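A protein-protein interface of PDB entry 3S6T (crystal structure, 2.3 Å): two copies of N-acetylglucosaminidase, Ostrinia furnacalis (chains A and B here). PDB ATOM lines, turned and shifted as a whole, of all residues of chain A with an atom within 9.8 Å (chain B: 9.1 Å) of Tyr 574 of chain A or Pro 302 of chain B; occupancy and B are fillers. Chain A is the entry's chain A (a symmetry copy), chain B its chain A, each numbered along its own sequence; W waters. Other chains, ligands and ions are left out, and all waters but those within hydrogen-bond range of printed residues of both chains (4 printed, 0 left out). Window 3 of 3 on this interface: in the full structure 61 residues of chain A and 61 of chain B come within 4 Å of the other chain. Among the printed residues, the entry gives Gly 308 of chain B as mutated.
Water W3 lies within hydrogen-bond range of the side-chain carboxylate (OE1) of Glu 301 of chain B (2.5 Å) and the backbone carbonyl oxygen (O) of Tyr 572 of chain A (3.0 Å).
Water W2 bridges ND2 of Asn 569 of chain A and NZ of Lys 299 of chain B.
Water W4 lies within hydrogen-bond range of the backbone NH of Ser 575 of chain A and the backbone NH of Gly 466 of chain B.
Water W1 lies within hydrogen-bond range of OH of Tyr 574 of chain A, N of Lys 304 of chain B and N of Trp 303 of chain B.
Printed residues of chain B within 4 Å of Gln 562 of chain A: Trp 464 (3.6 Å).
Tyr 574 of chain A touches just these residues of chain B: Glu 301 (2.6 Å), Pro 302 (3.8 Å), Trp 303 (3.1 Å) and Val 465 (3.9 Å).
Of chain B, only Lys 304 (3.0 Å), Val 465 (3.7 Å) and Gly 466 (3.8 Å) come within 4 Å of Ser 575 of chain A.
Printed residues of chain A within 4 Å of Lys 299 of chain B: Trp 565 and Tyr 572.
Of chain A, only Tyr 574 (2.6 Å) comes within 4 Å of Glu 301 of chain B.
Of chain A, only Tyr 574 comes within 4 Å of Pro 302 of chain B.
Of the printed residues of chain A, Lys 304 of chain B touches Ser 575.
No residue of chain A comes within 4 Å of Ser 305 of chain B.
Of the printed residues of chain A, Trp 464 of chain B touches Gln 562 (3.6 Å) and Pro 563 (3.4 Å).
The nearest residue of chain B that does not touch Tyr 574 of chain A is Gly 466 of chain B (4.6 Å).
The nearest residue of chain A that does not touch Pro 302 of chain B is Tyr 572 of chain A (7.6 Å).
The nearest printed residue of chain A that does not touch Val 465 of chain B is Cys 573 of chain A (4.4 Å).
Of the 20 printed residues of chain B, 11 touch a printed residue of chain A.
Printed residues of chain B that touch a printed residue of chain A: Lys 299, Glu 301, Pro 302, Trp 303, Lys 304, Pro 310, Pro 311, Trp 464, Val 465, Gly 466 and Ala 467.
Hydrophobic or aromatic side chains of chain A within 4 Å of the printed part of chain B: Trp 537, Pro 563, Trp 565, Tyr 572 and Tyr 574.
No position is printed for both chains.
Among the printed residues, merely in contact across the chains: Trp 537 of chain A with Gly 466 of chain B (3.5 Å), Trp 537 of chain A with Ala 467 of chain B (3.8 Å), Gln 562 of chain A with Trp 464 of chain B (3.6 Å), Pro 563 of chain A with Trp 464 of chain B (3.4 Å), Trp 565 of chain A with Lys 299 of chain B (3.99 Å), Trp 565 of chain A with Pro 311 of chain B (3.6 Å), Tyr 572 of chain A with Lys 299 of chain B (3.8 Å), Tyr 572 of chain A with Trp 303 of chain B (3.8 Å), Tyr 572 of chain A with Pro 310 of chain B (3.6 Å), Tyr 574 of chain A with Pro 302 of chain B (3.8 Å), Tyr 574 of chain A with Val 465 of chain B (3.9 Å), Ser 575 of chain A with Val 465 of chain B (3.7 Å) and Ser 575 of chain A with Gly 466 of chain B (3.8 Å).
NE1 of Trp 303 of chain B is in hydrogen-bond range of O of Tyr 574 of chain A, 3.1 Å away.
The side-chain carboxylate (OE2) of Glu 301 of chain B lies within hydrogen-bond range of the side-chain hydroxyl (OH) of Tyr 574 of chain A (2.6 Å).
NZ of Lys 304 of chain B is in hydrogen-bond range of OG of Ser 575 of chain A (3.0 Å).
The side-chain sulfur (SG) of Cys 312 of chain B forms a disulfide with the side-chain sulfur (SG) of Cys 307 of chain B (2.3 Å).
The side-chain carboxylate (OE1) of Glu 541 of chain A sits at hydrogen-bond distance from the side-chain amide nitrogen (NE2) of Gln 562 of chain A, 3.0 Å away.
SG of Cys 573 of chain A forms a disulfide with SG of Cys 566 of chain A.
NE1 of Trp 537 of chain A lies close to NE2 of Gln 538 of chain A.
O of Trp 565 of chain A lies close to OD1 of Asn 569 of chain A.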
ATOM      1  N   LYS A  16      -6.752 -27.947 -12.687  1.00  0.00           N
ATOM      2  CA  LYS A  16      -7.104 -26.693 -13.300  1.00  0.00           C
ATOM      3  C   LYS A  16      -8.494 -26.703 -13.878  1.00  0.00           C
ATOM      4  O   LYS A  16      -8.862 -27.598 -14.556  1.00  0.00           O
ATOM      5  CB  LYS A  16      -6.110 -26.357 -14.389  1.00  0.00           C
ATOM      6  CG  LYS A  16      -4.712 -26.263 -13.915  1.00  0.00           C
ATOM      7  CD  LYS A  16      -3.754 -26.110 -15.032  1.00  0.00           C
ATOM      8  CE  LYS A  16      -3.799 -27.282 -15.924  1.00  0.00           C
ATOM      9  NZ  LYS A  16      -2.546 -27.532 -16.594  1.00  0.00           N
ATOM     10  N   TRP A 537       3.976 -19.948  -2.953  1.00  0.00           N
ATOM     11  CA  TRP A 537       2.919 -19.079  -3.433  1.00  0.00           C
ATOM     12  C   TRP A 537       2.163 -19.648  -4.614  1.00  0.00           C
ATOM     13  O   TRP A 537       0.991 -19.489  -4.714  1.00  0.00           O
ATOM     14  CB  TRP A 537       3.424 -17.671  -3.723  1.00  0.00           C
ATOM     15  CG  TRP A 537       4.277 -17.473  -4.920  1.00  0.00           C
ATOM     16  CD1 TRP A 537       5.599 -17.369  -4.946  1.00  0.00           C
ATOM     17  CD2 TRP A 537       3.845 -17.300  -6.255  1.00  0.00           C
ATOM     18  NE1 TRP A 537       6.037 -17.172  -6.187  1.00  0.00           N
ATOM     19  CE2 TRP A 537       4.972 -17.115  -7.023  1.00  0.00           C
ATOM     20  CE3 TRP A 537       2.612 -17.289  -6.873  1.00  0.00           C
ATOM     21  CZ2 TRP A 537       4.916 -16.931  -8.365  1.00  0.00           C
ATOM     22  CZ3 TRP A 537       2.563 -17.125  -8.186  1.00  0.00           C
ATOM     23  CH2 TRP A 537       3.697 -16.942  -8.930  1.00  0.00           C
ATOM     24  N   GLN A 538       2.852 -20.334  -5.494  1.00  0.00           N
ATOM     25  CA  GLN A 538       2.221 -20.863  -6.671  1.00  0.00           C
ATOM     26  C   GLN A 538       1.153 -21.872  -6.374  1.00  0.00           C
ATOM     27  O   GLN A 538       0.243 -22.009  -7.106  1.00  0.00           O
ATOM     28  CB  GLN A 538       3.210 -21.290  -7.739  1.00  0.00           C
ATOM     29  CG  GLN A 538       4.507 -21.812  -7.266  1.00  0.00           C
ATOM     30  CD  GLN A 538       5.563 -20.764  -7.063  1.00  0.00           C
ATOM     31  OE1 GLN A 538       6.109 -20.244  -7.988  1.00  0.00           O
ATOM     32  NE2 GLN A 538       5.886 -20.512  -5.849  1.00  0.00           N
ATOM     33  N   GLU A 541      -1.887 -19.805  -5.409  1.00  0.00           N
ATOM     34  CA  GLU A 541      -2.270 -18.771  -6.355  1.00  0.00           C
ATOM     35  C   GLU A 541      -3.724 -18.700  -6.792  1.00  0.00           C
ATOM     36  O   GLU A 541      -4.284 -17.643  -6.761  1.00  0.00           O
ATOM     37  CB  GLU A 541      -1.361 -18.836  -7.580  1.00  0.00           C
ATOM     38  CG  GLU A 541      -1.844 -18.117  -8.784  1.00  0.00           C
ATOM     39  CD  GLU A 541      -0.922 -18.200  -9.991  1.00  0.00           C
ATOM     40  OE1 GLU A 541      -0.822 -17.248 -10.732  1.00  0.00           O
ATOM     41  OE2 GLU A 541      -0.319 -19.214 -10.234  1.00  0.00           O
ATOM     42  N   TYR A 542      -4.336 -19.799  -7.158  1.00  0.00           N
ATOM     43  CA  TYR A 542      -5.711 -19.782  -7.555  1.00  0.00           C
ATOM     44  C   TYR A 542      -6.644 -19.317  -6.448  1.00  0.00           C
ATOM     45  O   TYR A 542      -7.524 -18.566  -6.691  1.00  0.00           O
ATOM     46  CB  TYR A 542      -6.153 -21.149  -8.059  1.00  0.00           C
ATOM     47  CG  TYR A 542      -5.343 -21.740  -9.177  1.00  0.00           C
ATOM     48  CD1 TYR A 542      -5.397 -23.080  -9.443  1.00  0.00           C
ATOM     49  CD2 TYR A 542      -4.536 -20.973  -9.957  1.00  0.00           C
ATOM     50  CE1 TYR A 542      -4.695 -23.615 -10.423  1.00  0.00           C
ATOM     51  CE2 TYR A 542      -3.824 -21.510 -10.941  1.00  0.00           C
ATOM     52  CZ  TYR A 542      -3.893 -22.838 -11.177  1.00  0.00           C
ATOM     53  OH  TYR A 542      -3.176 -23.394 -12.170  1.00  0.00           O
ATOM     54  N   GLN A 562      -4.382  -9.984 -11.139  1.00  0.00           N
ATOM     55  CA  GLN A 562      -4.259 -10.528 -12.463  1.00  0.00           C
ATOM     56  C   GLN A 562      -5.482 -10.258 -13.270  1.00  0.00           C
ATOM     57  O   GLN A 562      -6.460  -9.875 -12.759  1.00  0.00           O
ATOM     58  CB  GLN A 562      -4.077 -12.039 -12.387  1.00  0.00           C
ATOM     59  CG  GLN A 562      -2.886 -12.473 -11.616  1.00  0.00           C
ATOM     60  CD  GLN A 562      -2.627 -13.967 -11.612  1.00  0.00           C
ATOM     61  OE1 GLN A 562      -3.092 -14.699 -12.438  1.00  0.00           O
ATOM     62  NE2 GLN A 562      -1.846 -14.390 -10.683  1.00  0.00           N
ATOM     63  N   PRO A 563      -5.412 -10.475 -14.559  1.00  0.00           N
ATOM     64  CA  PRO A 563      -6.591 -10.334 -15.366  1.00  0.00           C
ATOM     65  C   PRO A 563      -7.588 -11.373 -14.945  1.00  0.00           C
ATOM     66  O   PRO A 563      -7.203 -12.449 -14.617  1.00  0.00           O
ATOM     67  CB  PRO A 563      -6.077 -10.645 -16.740  1.00  0.00           C
ATOM     68  CG  PRO A 563      -4.747 -10.319 -16.691  1.00  0.00           C
ATOM     69  CD  PRO A 563      -4.240 -10.644 -15.405  1.00  0.00           C
ATOM     70  N   TRP A 565      -9.376 -12.988 -16.741  1.00  0.00           N
ATOM     71  CA  TRP A 565      -9.295 -14.069 -17.667  1.00  0.00           C
ATOM     72  C   TRP A 565      -8.487 -15.195 -17.048  1.00  0.00           C
ATOM     73  O   TRP A 565      -8.789 -16.317 -17.249  1.00  0.00           O
ATOM     74  CB  TRP A 565      -8.718 -13.617 -19.008  1.00  0.00           C
ATOM     75  CG  TRP A 565      -8.771 -14.644 -20.047  1.00  0.00           C
ATOM     76  CD1 TRP A 565      -9.771 -14.863 -20.887  1.00  0.00           C
ATOM     77  CD2 TRP A 565      -7.791 -15.625 -20.333  1.00  0.00           C
ATOM     78  NE1 TRP A 565      -9.509 -15.904 -21.671  1.00  0.00           N
ATOM     79  CE2 TRP A 565      -8.286 -16.401 -21.355  1.00  0.00           C
ATOM     80  CE3 TRP A 565      -6.543 -15.929 -19.812  1.00  0.00           C
ATOM     81  CZ2 TRP A 565      -7.585 -17.449 -21.881  1.00  0.00           C
ATOM     82  CZ3 TRP A 565      -5.858 -16.964 -20.338  1.00  0.00           C
ATOM     83  CH2 TRP A 565      -6.369 -17.703 -21.363  1.00  0.00           C
ATOM     84  N   CYS A 566      -7.463 -14.871 -16.290  1.00  0.00           N
ATOM     85  CA  CYS A 566      -6.638 -15.857 -15.625  1.00  0.00           C
ATOM     86  C   CYS A 566      -7.393 -16.666 -14.598  1.00  0.00           C
ATOM     87  O   CYS A 566      -7.202 -17.829 -14.476  1.00  0.00           O
ATOM     88  CB  CYS A 566      -5.389 -15.218 -15.011  1.00  0.00           C
ATOM     89  SG  CYS A 566      -4.368 -14.364 -16.118  1.00  0.00           S
ATOM     90  N   ASN A 569      -9.395 -19.009 -16.459  1.00  0.00           N
ATOM     91  CA  ASN A 569      -8.635 -19.931 -17.260  1.00  0.00           C
ATOM     92  C   ASN A 569      -7.337 -20.371 -16.635  1.00  0.00           C
ATOM     93  O   ASN A 569      -6.295 -20.055 -17.107  1.00  0.00           O
ATOM     94  CB  ASN A 569      -8.377 -19.315 -18.639  1.00  0.00           C
ATOM     95  CG  ASN A 569      -9.624 -19.190 -19.455  1.00  0.00           C
ATOM     96  OD1 ASN A 569     -10.252 -18.192 -19.453  1.00  0.00           O
ATOM     97  ND2 ASN A 569      -9.981 -20.219 -20.129  1.00  0.00           N
ATOM     98  N   GLU A 570      -7.438 -21.153 -15.586  1.00  0.00           N
ATOM     99  CA  GLU A 570      -6.311 -21.614 -14.827  1.00  0.00           C
ATOM    100  C   GLU A 570      -5.271 -22.406 -15.601  1.00  0.00           C
ATOM    101  O   GLU A 570      -5.579 -23.280 -16.344  1.00  0.00           O
ATOM    102  CB  GLU A 570      -6.822 -22.457 -13.662  1.00  0.00           C
ATOM    103  CG  GLU A 570      -7.408 -21.663 -12.544  1.00  0.00           C
ATOM    104  CD  GLU A 570      -8.173 -22.467 -11.555  1.00  0.00           C
ATOM    105  OE1 GLU A 570      -8.673 -21.891 -10.623  1.00  0.00           O
ATOM    106  OE2 GLU A 570      -8.292 -23.666 -11.681  1.00  0.00           O
ATOM    107  N   GLY A 571      -4.025 -22.034 -15.388  1.00  0.00           N
ATOM    108  CA  GLY A 571      -2.874 -22.619 -16.016  1.00  0.00           C
ATOM    109  C   GLY A 571      -2.391 -21.933 -17.261  1.00  0.00           C
ATOM    110  O   GLY A 571      -1.306 -22.165 -17.690  1.00  0.00           O
ATOM    111  N   TYR A 572      -3.216 -21.101 -17.841  1.00  0.00           N
ATOM    112  CA  TYR A 572      -2.834 -20.309 -18.975  1.00  0.00           C
ATOM    113  C   TYR A 572      -1.907 -19.128 -18.737  1.00  0.00           C
ATOM    114  O   TYR A 572      -1.207 -18.739 -19.609  1.00  0.00           O
ATOM    115  CB  TYR A 572      -4.009 -19.946 -19.852  1.00  0.00           C
ATOM    116  CG  TYR A 572      -4.540 -21.099 -20.617  1.00  0.00           C
ATOM    117  CD1 TYR A 572      -5.600 -21.823 -20.151  1.00  0.00           C
ATOM    118  CD2 TYR A 572      -3.982 -21.475 -21.795  1.00  0.00           C
ATOM    119  CE1 TYR A 572      -6.072 -22.865 -20.822  1.00  0.00           C
ATOM    120  CE2 TYR A 572      -4.451 -22.517 -22.468  1.00  0.00           C
ATOM    121  CZ  TYR A 572      -5.505 -23.210 -21.983  1.00  0.00           C
ATOM    122  OH  TYR A 572      -5.998 -24.257 -22.663  1.00  0.00           O
ATOM    123  N   CYS A 573      -1.935 -18.534 -17.572  1.00  0.00           N
ATOM    124  CA  CYS A 573      -1.089 -17.416 -17.297  1.00  0.00           C
ATOM    125  C   CYS A 573      -0.034 -17.868 -16.321  1.00  0.00           C
ATOM    126  O   CYS A 573      -0.330 -18.148 -15.215  1.00  0.00           O
ATOM    127  CB  CYS A 573      -1.904 -16.293 -16.692  1.00  0.00           C
ATOM    128  SG  CYS A 573      -3.329 -15.783 -17.559  1.00  0.00           S
ATOM    129  N   TYR A 574       1.205 -17.950 -16.745  1.00  0.00           N
ATOM    130  CA  TYR A 574       2.265 -18.433 -15.896  1.00  0.00           C
ATOM    131  C   TYR A 574       3.612 -17.934 -16.347  1.00  0.00           C
ATOM    132  O   TYR A 574       3.756 -17.489 -17.437  1.00  0.00           O
ATOM    133  CB  TYR A 574       2.304 -19.946 -15.952  1.00  0.00           C
ATOM    134  CG  TYR A 574       2.634 -20.464 -17.314  1.00  0.00           C
ATOM    135  CD1 TYR A 574       1.652 -20.740 -18.218  1.00  0.00           C
ATOM    136  CD2 TYR A 574       3.932 -20.665 -17.700  1.00  0.00           C
ATOM    137  CE1 TYR A 574       1.946 -21.192 -19.450  1.00  0.00           C
ATOM    138  CE2 TYR A 574       4.231 -21.122 -18.933  1.00  0.00           C
ATOM    139  CZ  TYR A 574       3.234 -21.379 -19.800  1.00  0.00           C
ATOM    140  OH  TYR A 574       3.537 -21.810 -21.017  1.00  0.00           O
ATOM    141  N   SER A 575       4.600 -18.035 -15.483  1.00  0.00           N
ATOM    142  CA  SER A 575       5.962 -17.684 -15.801  1.00  0.00           C
ATOM    143  C   SER A 575       6.925 -18.087 -14.729  1.00  0.00           C
ATOM    144  O   SER A 575       7.855 -18.824 -14.994  1.00  0.00           O
ATOM    145  CB  SER A 575       6.113 -16.216 -16.044  1.00  0.00           C
ATOM    146  OG  SER A 575       7.438 -15.950 -16.313  1.00  0.00           O
ATOM    147  N   CYS B 297      -4.004 -19.078 -33.276  1.00  0.00           N
ATOM    148  CA  CYS B 297      -3.234 -19.089 -32.066  1.00  0.00           C
ATOM    149  C   CYS B 297      -3.913 -18.728 -30.772  1.00  0.00           C
ATOM    150  O   CYS B 297      -3.240 -18.446 -29.858  1.00  0.00           O
ATOM    151  CB  CYS B 297      -2.055 -18.172 -32.212  1.00  0.00           C
ATOM    152  SG  CYS B 297      -0.861 -18.744 -33.249  1.00  0.00           S
ATOM    153  N   LYS B 299      -4.896 -18.950 -27.323  1.00  0.00           N
ATOM    154  CA  LYS B 299      -4.448 -19.795 -26.251  1.00  0.00           C
ATOM    155  C   LYS B 299      -3.325 -20.708 -26.623  1.00  0.00           C
ATOM    156  O   LYS B 299      -3.159 -21.710 -26.014  1.00  0.00           O
ATOM    157  CB  LYS B 299      -5.591 -20.616 -25.702  1.00  0.00           C
ATOM    158  CG  LYS B 299      -6.459 -19.838 -24.877  1.00  0.00           C
ATOM    159  CD  LYS B 299      -7.805 -20.286 -25.009  1.00  0.00           C
ATOM    160  CE  LYS B 299      -8.100 -21.273 -24.007  1.00  0.00           C
ATOM    161  NZ  LYS B 299      -9.319 -21.893 -24.429  1.00  0.00           N
ATOM    162  N   ALA B 300      -2.527 -20.328 -27.596  1.00  0.00           N
ATOM    163  CA  ALA B 300      -1.411 -21.136 -28.015  1.00  0.00           C
ATOM    164  C   ALA B 300      -0.404 -21.325 -26.906  1.00  0.00           C
ATOM    165  O   ALA B 300      -0.110 -20.425 -26.211  1.00  0.00           O
ATOM    166  CB  ALA B 300      -0.752 -20.508 -29.189  1.00  0.00           C
ATOM    167  N   GLU B 301       0.111 -22.523 -26.753  1.00  0.00           N
ATOM    168  CA  GLU B 301       1.095 -22.818 -25.745  1.00  0.00           C
ATOM    169  C   GLU B 301       2.315 -23.435 -26.376  1.00  0.00           C
ATOM    170  O   GLU B 301       2.180 -24.175 -27.300  1.00  0.00           O
ATOM    171  CB  GLU B 301       0.524 -23.762 -24.732  1.00  0.00           C
ATOM    172  CG  GLU B 301      -0.229 -23.079 -23.664  1.00  0.00           C
ATOM    173  CD  GLU B 301       0.655 -22.309 -22.761  1.00  0.00           C
ATOM    174  OE1 GLU B 301       0.510 -21.120 -22.665  1.00  0.00           O
ATOM    175  OE2 GLU B 301       1.497 -22.893 -22.116  1.00  0.00           O
ATOM    176  N   PRO B 302       3.509 -23.142 -25.885  1.00  0.00           N
ATOM    177  CA  PRO B 302       3.759 -22.217 -24.793  1.00  0.00           C
ATOM    178  C   PRO B 302       3.588 -20.776 -25.207  1.00  0.00           C
ATOM    179  O   PRO B 302       4.092 -20.402 -26.225  1.00  0.00           O
ATOM    180  CB  PRO B 302       5.211 -22.495 -24.464  1.00  0.00           C
ATOM    181  CG  PRO B 302       5.754 -22.995 -25.630  1.00  0.00           C
ATOM    182  CD  PRO B 302       4.745 -23.773 -26.318  1.00  0.00           C
ATOM    183  N   TRP B 303       2.944 -19.977 -24.387  1.00  0.00           N
ATOM    184  CA  TRP B 303       2.604 -18.626 -24.759  1.00  0.00           C
ATOM    185  C   TRP B 303       3.766 -17.751 -25.108  1.00  0.00           C
ATOM    186  O   TRP B 303       3.673 -16.926 -25.968  1.00  0.00           O
ATOM    187  CB  TRP B 303       1.678 -17.957 -23.756  1.00  0.00           C
ATOM    188  CG  TRP B 303       2.250 -17.562 -22.466  1.00  0.00           C
ATOM    189  CD1 TRP B 303       2.162 -18.230 -21.313  1.00  0.00           C
ATOM    190  CD2 TRP B 303       2.954 -16.372 -22.181  1.00  0.00           C
ATOM    191  NE1 TRP B 303       2.774 -17.553 -20.331  1.00  0.00           N
ATOM    192  CE2 TRP B 303       3.271 -16.396 -20.843  1.00  0.00           C
ATOM    193  CE3 TRP B 303       3.351 -15.281 -22.939  1.00  0.00           C
ATOM    194  CZ2 TRP B 303       3.963 -15.389 -20.244  1.00  0.00           C
ATOM    195  CZ3 TRP B 303       4.036 -14.301 -22.345  1.00  0.00           C
ATOM    196  CH2 TRP B 303       4.340 -14.349 -21.017  1.00  0.00           C
ATOM    197  N   LYS B 304       4.879 -17.971 -24.448  1.00  0.00           N
ATOM    198  CA  LYS B 304       6.039 -17.166 -24.659  1.00  0.00           C
ATOM    199  C   LYS B 304       6.552 -17.241 -26.068  1.00  0.00           C
ATOM    200  O   LYS B 304       7.118 -16.310 -26.551  1.00  0.00           O
ATOM    201  CB  LYS B 304       7.112 -17.485 -23.655  1.00  0.00           C
ATOM    202  CG  LYS B 304       7.246 -16.428 -22.621  1.00  0.00           C
ATOM    203  CD  LYS B 304       7.812 -16.977 -21.353  1.00  0.00           C
ATOM    204  CE  LYS B 304       7.837 -15.965 -20.262  1.00  0.00           C
ATOM    205  NZ  LYS B 304       8.395 -16.542 -19.065  1.00  0.00           N
ATOM    206  N   SER B 305       6.355 -18.368 -26.714  1.00  0.00           N
ATOM    207  CA  SER B 305       6.795 -18.537 -28.067  1.00  0.00           C
ATOM    208  C   SER B 305       6.020 -17.740 -29.078  1.00  0.00           C
ATOM    209  O   SER B 305       6.506 -17.495 -30.140  1.00  0.00           O
ATOM    210  CB  SER B 305       6.834 -19.999 -28.450  1.00  0.00           C
ATOM    211  OG  SER B 305       7.676 -20.713 -27.591  1.00  0.00           O
ATOM    212  N   TYR B 306       4.795 -17.396 -28.749  1.00  0.00           N
ATOM    213  CA  TYR B 306       3.888 -16.792 -29.690  1.00  0.00           C
ATOM    214  C   TYR B 306       3.398 -15.394 -29.411  1.00  0.00           C
ATOM    215  O   TYR B 306       2.790 -14.802 -30.249  1.00  0.00           O
ATOM    216  CB  TYR B 306       2.669 -17.689 -29.847  1.00  0.00           C
ATOM    217  CG  TYR B 306       2.994 -19.076 -30.256  1.00  0.00           C
ATOM    218  CD1 TYR B 306       3.161 -19.392 -31.569  1.00  0.00           C
ATOM    219  CD2 TYR B 306       3.159 -20.054 -29.333  1.00  0.00           C
ATOM    220  CE1 TYR B 306       3.477 -20.641 -31.949  1.00  0.00           C
ATOM    221  CE2 TYR B 306       3.479 -21.297 -29.696  1.00  0.00           C
ATOM    222  CZ  TYR B 306       3.632 -21.596 -31.010  1.00  0.00           C
ATOM    223  OH  TYR B 306       3.945 -22.855 -31.393  1.00  0.00           O
ATOM    224  N   CYS B 307       3.599 -14.880 -28.222  1.00  0.00           N
ATOM    225  CA  CYS B 307       3.117 -13.549 -27.940  1.00  0.00           C
ATOM    226  C   CYS B 307       3.750 -12.885 -26.753  1.00  0.00           C
ATOM    227  O   CYS B 307       4.475 -13.476 -26.019  1.00  0.00           O
ATOM    228  CB  CYS B 307       1.605 -13.489 -27.860  1.00  0.00           C
ATOM    229  SG  CYS B 307       0.949 -14.419 -26.598  1.00  0.00           S
ATOM    230  N   GLY B 308       3.493 -11.610 -26.627  1.00  0.00           N
ATOM    231  CA  GLY B 308       3.937 -10.830 -25.512  1.00  0.00           C
ATOM    232  C   GLY B 308       3.351 -11.200 -24.183  1.00  0.00           C
ATOM    233  O   GLY B 308       4.016 -11.116 -23.202  1.00  0.00           O
ATOM    234  N   GLU B 309       2.071 -11.536 -24.177  1.00  0.00           N
ATOM    235  CA  GLU B 309       1.367 -11.975 -23.008  1.00  0.00           C
ATOM    236  C   GLU B 309       0.176 -12.838 -23.332  1.00  0.00           C
ATOM    237  O   GLU B 309      -0.441 -12.684 -24.321  1.00  0.00           O
ATOM    238  CB  GLU B 309       0.906 -10.791 -22.183  1.00  0.00           C
ATOM    239  CG  GLU B 309      -0.339 -10.135 -22.663  1.00  0.00           C
ATOM    240  CD  GLU B 309      -0.515  -8.753 -22.115  1.00  0.00           C
ATOM    241  OE1 GLU B 309      -1.348  -8.549 -21.255  1.00  0.00           O
ATOM    242  OE2 GLU B 309       0.176  -7.871 -22.564  1.00  0.00           O
ATOM    243  N   PRO B 310      -0.153 -13.726 -22.431  1.00  0.00           N
ATOM    244  CA  PRO B 310      -1.288 -14.620 -22.568  1.00  0.00           C
ATOM    245  C   PRO B 310      -2.613 -13.970 -22.261  1.00  0.00           C
ATOM    246  O   PRO B 310      -2.672 -13.157 -21.398  1.00  0.00           O
ATOM    247  CB  PRO B 310      -0.983 -15.681 -21.540  1.00  0.00           C
ATOM    248  CG  PRO B 310      -0.231 -15.031 -20.575  1.00  0.00           C
ATOM    249  CD  PRO B 310       0.490 -13.899 -21.141  1.00  0.00           C
ATOM    250  N   PRO B 311      -3.665 -14.342 -22.947  1.00  0.00           N
ATOM    251  CA  PRO B 311      -3.614 -15.324 -24.007  1.00  0.00           C
ATOM    252  C   PRO B 311      -3.166 -14.813 -25.373  1.00  0.00           C
ATOM    253  O   PRO B 311      -3.430 -13.717 -25.726  1.00  0.00           O
ATOM    254  CB  PRO B 311      -5.052 -15.789 -24.085  1.00  0.00           C
ATOM    255  CG  PRO B 311      -5.818 -14.662 -23.702  1.00  0.00           C
ATOM    256  CD  PRO B 311      -5.035 -13.887 -22.726  1.00  0.00           C
ATOM    257  N   CYS B 312      -2.518 -15.668 -26.131  1.00  0.00           N
ATOM    258  CA  CYS B 312      -2.105 -15.412 -27.487  1.00  0.00           C
ATOM    259  C   CYS B 312      -3.317 -15.417 -28.387  1.00  0.00           C
ATOM    260  O   CYS B 312      -4.334 -15.897 -28.015  1.00  0.00           O
ATOM    261  CB  CYS B 312      -1.128 -16.477 -27.965  1.00  0.00           C
ATOM    262  SG  CYS B 312       0.432 -16.574 -27.166  1.00  0.00           S
ATOM    263  N   ALA B 353       5.581 -15.431 -35.482  1.00  0.00           N
ATOM    264  CA  ALA B 353       5.521 -16.837 -35.210  1.00  0.00           C
ATOM    265  C   ALA B 353       4.122 -17.344 -35.270  1.00  0.00           C
ATOM    266  O   ALA B 353       3.860 -18.417 -35.727  1.00  0.00           O
ATOM    267  CB  ALA B 353       6.096 -17.122 -33.875  1.00  0.00           C
ATOM    268  N   TRP B 464       2.404 -10.126 -12.601  1.00  0.00           N
ATOM    269  CA  TRP B 464       1.155 -10.850 -12.757  1.00  0.00           C
ATOM    270  C   TRP B 464       1.328 -12.250 -13.341  1.00  0.00           C
ATOM    271  O   TRP B 464       0.458 -13.065 -13.268  1.00  0.00           O
ATOM    272  CB  TRP B 464       0.073 -10.038 -13.452  1.00  0.00           C
ATOM    273  CG  TRP B 464       0.283  -9.711 -14.867  1.00  0.00           C
ATOM    274  CD1 TRP B 464       0.975  -8.691 -15.349  1.00  0.00           C
ATOM    275  CD2 TRP B 464      -0.246 -10.392 -15.991  1.00  0.00           C
ATOM    276  NE1 TRP B 464       0.946  -8.685 -16.672  1.00  0.00           N
ATOM    277  CE2 TRP B 464       0.185  -9.718 -17.106  1.00  0.00           C
ATOM    278  CE3 TRP B 464      -1.046 -11.515 -16.159  1.00  0.00           C
ATOM    279  CZ2 TRP B 464      -0.135 -10.112 -18.366  1.00  0.00           C
ATOM    280  CZ3 TRP B 464      -1.362 -11.896 -17.414  1.00  0.00           C
ATOM    281  CH2 TRP B 464      -0.903 -11.198 -18.498  1.00  0.00           C
ATOM    282  N   VAL B 465       2.480 -12.502 -13.909  1.00  0.00           N
ATOM    283  CA  VAL B 465       2.887 -13.824 -14.302  1.00  0.00           C
ATOM    284  C   VAL B 465       4.209 -14.046 -13.616  1.00  0.00           C
ATOM    285  O   VAL B 465       5.106 -13.276 -13.745  1.00  0.00           O
ATOM    286  CB  VAL B 465       2.998 -14.041 -15.820  1.00  0.00           C
ATOM    287  CG1 VAL B 465       1.706 -13.830 -16.493  1.00  0.00           C
ATOM    288  CG2 VAL B 465       4.010 -13.168 -16.405  1.00  0.00           C
ATOM    289  N   GLY B 466       4.310 -15.103 -12.850  1.00  0.00           N
ATOM    290  CA  GLY B 466       5.521 -15.354 -12.129  1.00  0.00           C
ATOM    291  C   GLY B 466       5.641 -14.465 -10.930  1.00  0.00           C
ATOM    292  O   GLY B 466       4.690 -13.932 -10.479  1.00  0.00           O
ATOM    293  N   ALA B 467       6.836 -14.323 -10.420  1.00  0.00           N
ATOM    294  CA  ALA B 467       7.069 -13.520  -9.256  1.00  0.00           C
ATOM    295  C   ALA B 467       7.907 -12.320  -9.577  1.00  0.00           C
ATOM    296  O   ALA B 467       8.297 -12.161 -10.672  1.00  0.00           O
ATOM    297  CB  ALA B 467       7.638 -14.323  -8.177  1.00  0.00           C
HETATM  298  O   HOH W   1       5.300 -19.628 -21.883  1.00  0.00           O
HETATM  299  O   HOH W   2     -10.581 -19.448 -22.850  1.00  0.00           O
HETATM  300  O   HOH W   3      -1.306 -19.392 -22.498  1.00  0.00           O
HETATM  301  O   HOH W   4       3.700 -18.336 -12.736  1.00  0.00           O
